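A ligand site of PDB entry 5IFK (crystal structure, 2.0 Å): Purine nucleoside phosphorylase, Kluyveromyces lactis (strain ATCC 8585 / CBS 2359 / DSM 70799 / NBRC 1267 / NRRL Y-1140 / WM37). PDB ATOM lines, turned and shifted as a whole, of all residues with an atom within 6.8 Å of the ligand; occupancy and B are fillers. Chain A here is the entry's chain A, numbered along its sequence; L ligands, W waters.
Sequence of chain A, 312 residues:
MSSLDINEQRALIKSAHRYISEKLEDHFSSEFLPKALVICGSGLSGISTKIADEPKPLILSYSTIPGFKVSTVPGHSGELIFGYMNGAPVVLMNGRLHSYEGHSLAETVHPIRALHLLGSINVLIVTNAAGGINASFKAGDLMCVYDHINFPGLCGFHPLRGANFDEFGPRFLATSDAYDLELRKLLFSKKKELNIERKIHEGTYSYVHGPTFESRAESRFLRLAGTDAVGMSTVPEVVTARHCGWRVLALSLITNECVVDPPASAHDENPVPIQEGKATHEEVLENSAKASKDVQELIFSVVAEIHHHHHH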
ATOM      1  N   ASN A 128     -24.572 -16.308   7.064  1.00  0.00           N
ATOM      2  CA  ASN A 128     -24.307 -16.615   5.658  1.00  0.00           C
ATOM      3  C   ASN A 128     -24.695 -15.451   4.774  1.00  0.00           C
ATOM      4  O   ASN A 128     -25.383 -14.525   5.204  1.00  0.00           O
ATOM      5  CB  ASN A 128     -25.074 -17.873   5.216  1.00  0.00           C
ATOM      6  CG  ASN A 128     -26.584 -17.753   5.421  1.00  0.00           C
ATOM      7  OD1 ASN A 128     -27.237 -16.866   4.876  1.00  0.00           O
ATOM      8  ND2 ASN A 128     -27.144 -18.658   6.220  1.00  0.00           N
ATOM      9  N   ALA A 129     -24.278 -15.501   3.512  1.00  0.00           N
ATOM     10  CA  ALA A 129     -24.766 -14.545   2.531  1.00  0.00           C
ATOM     11  C   ALA A 129     -26.006 -15.138   1.869  1.00  0.00           C
ATOM     12  O   ALA A 129     -26.115 -16.357   1.722  1.00  0.00           O
ATOM     13  CB  ALA A 129     -23.689 -14.231   1.511  1.00  0.00           C
ATOM     14  N   ALA A 130     -26.948 -14.291   1.480  1.00  0.00           N
ATOM     15  CA  ALA A 130     -28.128 -14.781   0.788  1.00  0.00           C
ATOM     16  C   ALA A 130     -28.612 -13.799  -0.259  1.00  0.00           C
ATOM     17  O   ALA A 130     -28.439 -12.610  -0.119  1.00  0.00           O
ATOM     18  CB  ALA A 130     -29.250 -15.084   1.779  1.00  0.00           C
ATOM     19  N   GLY A 131     -29.241 -14.306  -1.313  1.00  0.00           N
ATOM     20  CA  GLY A 131     -29.879 -13.454  -2.292  1.00  0.00           C
ATOM     21  C   GLY A 131     -31.247 -13.110  -1.773  1.00  0.00           C
ATOM     22  O   GLY A 131     -31.948 -13.964  -1.230  1.00  0.00           O
ATOM     23  N   GLY A 132     -31.631 -11.847  -1.921  1.00  0.00           N
ATOM     24  CA  GLY A 132     -32.955 -11.429  -1.514  1.00  0.00           C
ATOM     25  C   GLY A 132     -34.036 -11.885  -2.484  1.00  0.00           C
ATOM     26  O   GLY A 132     -33.990 -11.567  -3.682  1.00  0.00           O
ATOM     27  N   ILE A 133     -35.013 -12.627  -1.982  1.00  0.00           N
ATOM     28  CA  ILE A 133     -36.093 -13.114  -2.827  1.00  0.00           C
ATOM     29  C   ILE A 133     -37.367 -12.313  -2.553  1.00  0.00           C
ATOM     30  O   ILE A 133     -38.095 -11.947  -3.475  1.00  0.00           O
ATOM     31  CB  ILE A 133     -36.339 -14.625  -2.613  1.00  0.00           C
ATOM     32  CG1 ILE A 133     -35.157 -15.439  -3.135  1.00  0.00           C
ATOM     33  CG2 ILE A 133     -37.591 -15.072  -3.346  1.00  0.00           C
ATOM     34  CD1 ILE A 133     -35.082 -15.494  -4.673  1.00  0.00           C
ATOM     35  N   TYR A 205     -35.580 -18.896   5.014  1.00  0.00           N
ATOM     36  CA  TYR A 205     -34.367 -19.097   4.237  1.00  0.00           C
ATOM     37  C   TYR A 205     -34.493 -20.383   3.435  1.00  0.00           C
ATOM     38  O   TYR A 205     -34.778 -21.426   4.004  1.00  0.00           O
ATOM     39  CB  TYR A 205     -33.147 -19.164   5.165  1.00  0.00           C
ATOM     40  CG  TYR A 205     -31.821 -19.512   4.512  1.00  0.00           C
ATOM     41  CD1 TYR A 205     -30.983 -18.523   3.994  1.00  0.00           C
ATOM     42  CD2 TYR A 205     -31.379 -20.826   4.429  1.00  0.00           C
ATOM     43  CE1 TYR A 205     -29.759 -18.837   3.409  1.00  0.00           C
ATOM     44  CE2 TYR A 205     -30.169 -21.151   3.832  1.00  0.00           C
ATOM     45  CZ  TYR A 205     -29.364 -20.155   3.337  1.00  0.00           C
ATOM     46  OH  TYR A 205     -28.155 -20.491   2.766  1.00  0.00           O
ATOM     47  N   VAL A 208     -30.491 -23.973  -1.400  1.00  0.00           N
ATOM     48  CA  VAL A 208     -30.350 -24.611  -2.703  1.00  0.00           C
ATOM     49  C   VAL A 208     -28.887 -25.006  -2.832  1.00  0.00           C
ATOM     50  O   VAL A 208     -28.034 -24.446  -2.133  1.00  0.00           O
ATOM     51  CB  VAL A 208     -30.779 -23.699  -3.874  1.00  0.00           C
ATOM     52  CG1 VAL A 208     -32.226 -23.246  -3.706  1.00  0.00           C
ATOM     53  CG2 VAL A 208     -29.864 -22.484  -3.976  1.00  0.00           C
ATOM     54  N   GLY A 210     -26.503 -24.795  -5.378  1.00  0.00           N
ATOM     55  CA  GLY A 210     -25.496 -24.002  -6.087  1.00  0.00           C
ATOM     56  C   GLY A 210     -24.675 -24.884  -6.995  1.00  0.00           C
ATOM     57  O   GLY A 210     -25.034 -26.039  -7.186  1.00  0.00           O
ATOM     58  N   THR A 212     -24.441 -22.293  -9.119  1.00  0.00           N
ATOM     59  CA  THR A 212     -25.038 -21.251  -9.974  1.00  0.00           C
ATOM     60  C   THR A 212     -25.877 -20.323  -9.124  1.00  0.00           C
ATOM     61  O   THR A 212     -26.458 -20.746  -8.132  1.00  0.00           O
ATOM     62  CB  THR A 212     -25.944 -21.836 -11.076  1.00  0.00           C
ATOM     63  OG1 THR A 212     -26.815 -22.838 -10.520  1.00  0.00           O
ATOM     64  CG2 THR A 212     -25.090 -22.432 -12.211  1.00  0.00           C
ATOM     65  N   PHE A 213     -25.931 -19.046  -9.498  1.00  0.00           N
ATOM     66  CA  PHE A 213     -26.967 -18.142  -9.022  1.00  0.00           C
ATOM     67  C   PHE A 213     -28.267 -18.453  -9.764  1.00  0.00           C
ATOM     68  O   PHE A 213     -28.224 -18.905 -10.906  1.00  0.00           O
ATOM     69  CB  PHE A 213     -26.585 -16.673  -9.245  1.00  0.00           C
ATOM     70  CG  PHE A 213     -25.373 -16.219  -8.481  1.00  0.00           C
ATOM     71  CD1 PHE A 213     -25.370 -16.207  -7.101  1.00  0.00           C
ATOM     72  CD2 PHE A 213     -24.248 -15.753  -9.162  1.00  0.00           C
ATOM     73  CE1 PHE A 213     -24.249 -15.765  -6.394  1.00  0.00           C
ATOM     74  CE2 PHE A 213     -23.143 -15.308  -8.470  1.00  0.00           C
ATOM     75  CZ  PHE A 213     -23.138 -15.310  -7.088  1.00  0.00           C
ATOM     76  N   GLU A 214     -29.397 -18.184  -9.131  1.00  0.00           N
ATOM     77  CA  GLU A 214     -30.702 -18.594  -9.668  1.00  0.00           C
ATOM     78  C   GLU A 214     -31.054 -17.877 -10.951  1.00  0.00           C
ATOM     79  O   GLU A 214     -30.808 -16.673 -11.099  1.00  0.00           O
ATOM     80  CB  GLU A 214     -31.813 -18.341  -8.635  1.00  0.00           C
ATOM     81  CG  GLU A 214     -31.675 -19.150  -7.357  1.00  0.00           C
ATOM     82  CD  GLU A 214     -30.513 -18.678  -6.490  1.00  0.00           C
ATOM     83  OE1 GLU A 214     -29.918 -19.528  -5.795  1.00  0.00           O
ATOM     84  OE2 GLU A 214     -30.177 -17.466  -6.513  1.00  0.00           O
ATOM     85  N   SER A 219     -35.826 -17.990  -9.272  1.00  0.00           N
ATOM     86  CA  SER A 219     -36.097 -17.053  -8.170  1.00  0.00           C
ATOM     87  C   SER A 219     -37.589 -16.840  -7.979  1.00  0.00           C
ATOM     88  O   SER A 219     -38.099 -16.771  -6.845  1.00  0.00           O
ATOM     89  CB  SER A 219     -35.426 -15.702  -8.407  1.00  0.00           C
ATOM     90  OG  SER A 219     -34.030 -15.850  -8.471  1.00  0.00           O
ATOM     91  N   VAL A 230     -32.388 -16.700  -0.300  1.00  0.00           N
ATOM     92  CA  VAL A 230     -31.863 -17.988  -0.757  1.00  0.00           C
ATOM     93  C   VAL A 230     -30.358 -18.046  -0.602  1.00  0.00           C
ATOM     94  O   VAL A 230     -29.665 -17.079  -0.871  1.00  0.00           O
ATOM     95  CB  VAL A 230     -32.234 -18.262  -2.236  1.00  0.00           C
ATOM     96  CG1 VAL A 230     -31.786 -17.099  -3.136  1.00  0.00           C
ATOM     97  CG2 VAL A 230     -31.625 -19.587  -2.710  1.00  0.00           C
ATOM     98  N   GLY A 231     -29.846 -19.181  -0.150  1.00  0.00           N
ATOM     99  CA  GLY A 231     -28.404 -19.352  -0.075  1.00  0.00           C
ATOM    100  C   GLY A 231     -27.973 -20.785  -0.314  1.00  0.00           C
ATOM    101  O   GLY A 231     -28.824 -21.685  -0.425  1.00  0.00           O
ATOM    102  N   MET A 232     -26.667 -20.994  -0.377  1.00  0.00           N
ATOM    103  CA  MET A 232     -26.118 -22.293  -0.730  1.00  0.00           C
ATOM    104  C   MET A 232     -25.526 -23.014   0.475  1.00  0.00           C
ATOM    105  O   MET A 232     -24.704 -23.905   0.304  1.00  0.00           O
ATOM    106  CB  MET A 232     -25.027 -22.121  -1.799  1.00  0.00           C
ATOM    107  CG  MET A 232     -25.450 -21.338  -3.014  1.00  0.00           C
ATOM    108  SD  MET A 232     -24.068 -21.030  -4.132  1.00  0.00           S
ATOM    109  CE  MET A 232     -24.891 -20.091  -5.424  1.00  0.00           C
ATOM    110  N   SER A 233     -25.915 -22.616   1.681  1.00  0.00           N
ATOM    111  CA  SER A 233     -25.305 -23.182   2.896  1.00  0.00           C
ATOM    112  C   SER A 233     -26.277 -23.274   4.058  1.00  0.00           C
ATOM    113  O   SER A 233     -27.486 -23.096   3.886  1.00  0.00           O
ATOM    114  CB  SER A 233     -24.088 -22.354   3.322  1.00  0.00           C
ATOM    115  OG  SER A 233     -24.490 -21.113   3.882  1.00  0.00           O
ATOM    116  N   LEU A 253     -27.125 -12.369   5.576  1.00  0.00           N
ATOM    117  CA  LEU A 253     -26.804 -11.072   4.990  1.00  0.00           C
ATOM    118  C   LEU A 253     -27.390 -11.020   3.599  1.00  0.00           C
ATOM    119  O   LEU A 253     -27.063 -11.873   2.763  1.00  0.00           O
ATOM    120  CB  LEU A 253     -25.292 -10.842   4.895  1.00  0.00           C
ATOM    121  CG  LEU A 253     -24.490 -10.467   6.128  1.00  0.00           C
ATOM    122  CD1 LEU A 253     -24.373 -11.675   7.076  1.00  0.00           C
ATOM    123  CD2 LEU A 253     -23.119 -10.002   5.661  1.00  0.00           C
ATOM    124  N   ILE A 254     -28.262 -10.067   3.326  1.00  0.00           N
ATOM    125  CA  ILE A 254     -28.785  -9.958   1.977  1.00  0.00           C
ATOM    126  C   ILE A 254     -27.723  -9.249   1.146  1.00  0.00           C
ATOM    127  O   ILE A 254     -27.501  -8.044   1.303  1.00  0.00           O
ATOM    128  CB  ILE A 254     -30.117  -9.214   1.926  1.00  0.00           C
ATOM    129  CG1 ILE A 254     -31.144  -9.889   2.858  1.00  0.00           C
ATOM    130  CG2 ILE A 254     -30.632  -9.132   0.491  1.00  0.00           C
ATOM    131  CD1 ILE A 254     -31.357 -11.391   2.543  1.00  0.00           C
ATOM    132  N   THR A 255     -27.026 -10.008   0.295  1.00  0.00           N
ATOM    133  CA  THR A 255     -25.876  -9.460  -0.435  1.00  0.00           C
ATOM    134  C   THR A 255     -26.237  -8.938  -1.813  1.00  0.00           C
ATOM    135  O   THR A 255     -25.444  -8.239  -2.443  1.00  0.00           O
ATOM    136  CB  THR A 255     -24.767 -10.510  -0.606  1.00  0.00           C
ATOM    137  OG1 THR A 255     -25.327 -11.706  -1.186  1.00  0.00           O
ATOM    138  CG2 THR A 255     -24.155 -10.832   0.738  1.00  0.00           C
ATOM    139  N   ASN A 256     -27.423  -9.299  -2.270  1.00  0.00           N
ATOM    140  CA  ASN A 256     -27.862  -8.956  -3.618  1.00  0.00           C
ATOM    141  C   ASN A 256     -29.363  -9.209  -3.730  1.00  0.00           C
ATOM    142  O   ASN A 256     -29.938  -9.983  -2.964  1.00  0.00           O
ATOM    143  CB  ASN A 256     -27.092  -9.779  -4.658  1.00  0.00           C
ATOM    144  CG  ASN A 256     -27.234 -11.264  -4.458  1.00  0.00           C
ATOM    145  OD1 ASN A 256     -26.658 -11.843  -3.532  1.00  0.00           O
ATOM    146  ND2 ASN A 256     -28.011 -11.920  -5.329  1.00  0.00           N
ATOM    147  N   GLU A 257     -29.997  -8.557  -4.699  1.00  0.00           N
ATOM    148  CA  GLU A 257     -31.419  -8.750  -4.904  1.00  0.00           C
ATOM    149  C   GLU A 257     -31.591  -9.651  -6.119  1.00  0.00           C
ATOM    150  O   GLU A 257     -31.158  -9.303  -7.204  1.00  0.00           O
ATOM    151  CB  GLU A 257     -32.134  -7.396  -5.090  1.00  0.00           C
ATOM    152  CG  GLU A 257     -32.018  -6.486  -3.859  1.00  0.00           C
ATOM    153  CD  GLU A 257     -32.196  -5.000  -4.179  1.00  0.00           C
ATOM    154  OE1 GLU A 257     -32.985  -4.668  -5.088  1.00  0.00           O
ATOM    155  OE2 GLU A 257     -31.526  -4.165  -3.509  1.00  0.00           O
ATOM    156  N   CYS A 258     -32.196 -10.812  -5.923  1.00  0.00           N
ATOM    157  CA  CYS A 258     -32.349 -11.731  -7.037  1.00  0.00           C
ATOM    158  C   CYS A 258     -33.190 -11.118  -8.141  1.00  0.00           C
ATOM    159  O   CYS A 258     -34.198 -10.433  -7.889  1.00  0.00           O
ATOM    160  CB  CYS A 258     -32.955 -13.042  -6.551  1.00  0.00           C
ATOM    161  SG  CYS A 258     -31.969 -13.790  -5.225  1.00  0.00           S
ATOM    162  N   ALA A 279     -26.306 -11.297 -10.730  1.00  0.00           N
ATOM    163  CA  ALA A 279     -25.538 -11.570  -9.516  1.00  0.00           C
ATOM    164  C   ALA A 279     -24.087 -11.893  -9.877  1.00  0.00           C
ATOM    165  O   ALA A 279     -23.819 -12.556 -10.884  1.00  0.00           O
ATOM    166  CB  ALA A 279     -26.153 -12.711  -8.718  1.00  0.00           C
ATOM    167  N   THR A 280     -23.165 -11.386  -9.056  1.00  0.00           N
ATOM    168  CA  THR A 280     -21.754 -11.707  -9.182  1.00  0.00           C
ATOM    169  C   THR A 280     -21.157 -11.990  -7.799  1.00  0.00           C
ATOM    170  O   THR A 280     -21.609 -11.436  -6.794  1.00  0.00           O
ATOM    171  CB  THR A 280     -20.933 -10.568  -9.831  1.00  0.00           C
ATOM    172  OG1 THR A 280     -21.050  -9.385  -9.032  1.00  0.00           O
ATOM    173  CG2 THR A 280     -21.408 -10.283 -11.251  1.00  0.00           C
ATOM    174  N   VAL A 284     -21.272 -10.023  -3.933  1.00  0.00           N
ATOM    175  CA  VAL A 284     -21.491 -10.761  -2.702  1.00  0.00           C
ATOM    176  C   VAL A 284     -20.381 -10.424  -1.687  1.00  0.00           C
ATOM    177  O   VAL A 284     -20.664 -10.108  -0.530  1.00  0.00           O
ATOM    178  CB  VAL A 284     -21.534 -12.288  -2.940  1.00  0.00           C
ATOM    179  CG1 VAL A 284     -21.598 -13.036  -1.619  1.00  0.00           C
ATOM    180  CG2 VAL A 284     -22.735 -12.637  -3.821  1.00  0.00           C
HETATM  181  N1  LIG L   1     -28.320 -17.010  -4.715  1.00  0.00           N
HETATM  182  C1  LIG L   1     -27.792 -18.043  -3.938  1.00  0.00           C
HETATM  183  N2  LIG L   1     -26.896 -17.885  -2.978  1.00  0.00           N
HETATM  184  C2  LIG L   1     -26.507 -16.567  -2.780  1.00  0.00           C
HETATM  185  C3  LIG L   1     -27.021 -15.487  -3.545  1.00  0.00           C
HETATM  186  C4  LIG L   1     -27.973 -15.647  -4.571  1.00  0.00           C
HETATM  187  O1  LIG L   1     -28.465 -14.777  -5.266  1.00  0.00           O
HETATM  188  N3  LIG L   1     -26.399 -14.349  -3.069  1.00  0.00           N
HETATM  189  C5  LIG L   1     -25.534 -14.733  -2.047  1.00  0.00           C
HETATM  190  N4  LIG L   1     -25.565 -16.097  -1.844  1.00  0.00           N
HETATM  191  O   HOH W   1     -29.661 -14.877  -7.803  1.00  0.00           O
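The side-chain amide oxygen (OD1) of Asn 256 sits at hydrogen-bond distance from a nitrogen (N3) of the ligand, 2.6 Å away. A nitrogen (N1) of the ligand lies within hydrogen-bond range of the side-chain carboxylate of Glu 214 (2.6 Å). OG1 of Thr 255 lies close to N3 of the ligand (3.4 Å). The backbone NH (N) of Gly 131 sits close to a nitrogen (N3) of the ligand, at 3.3 Å. SG of Cys 258 lies within hydrogen-bond range of O1 of the ligand.
OG1 of Thr 255 sits at hydrogen-bond distance from OD1 of Asn 256. O of Asn 256 is in hydrogen-bond range of N of Gly 132 (2.7 Å). O of Ala 130 is in hydrogen-bond range of N of Thr 255 (3.0 Å). O of Val 230 is in hydrogen-bond range of N of Gly 131, at 2.8 Å. The backbone carbonyl oxygen (O) of Gly 231 lies within hydrogen-bond range of the backbone NH (N) of Val 208, 3.0 Å away. The backbone carbonyl oxygen (O) of Gly 231 sits close to the side-chain hydroxyl (OH) of Tyr 205 (3.5 Å). The backbone carbonyl oxygen (O) of Leu 253 sits at hydrogen-bond distance from the backbone NH (N) of Ala 130 (2.7 Å). O of Gly 132 sits at hydrogen-bond distance from N of Cys 258, 3.0 Å away.
Ala 129 touches the ligand (O to N4, 3.6 Å). C of Ala 130 touches N3 of the ligand (3.6 Å). CD1 of Phe 213 touches C4 of the ligand (3.7 Å). Val 230 touches the ligand (O to N2, 3.6 Å). Gly 231 touches the ligand (CA to N2, 3.6 Å). Met 232 touches the ligand. Val 284 touches the ligand (CG2 to C5, 3.9 Å). Of the 26 residues printed, 12 come within 4 Å of the ligand.
Water W1 lies within hydrogen-bond range of O1 of the ligand (2.8 Å), OE2 of Glu 214 (2.9 Å) and SG of Cys 258 (3.6 Å).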
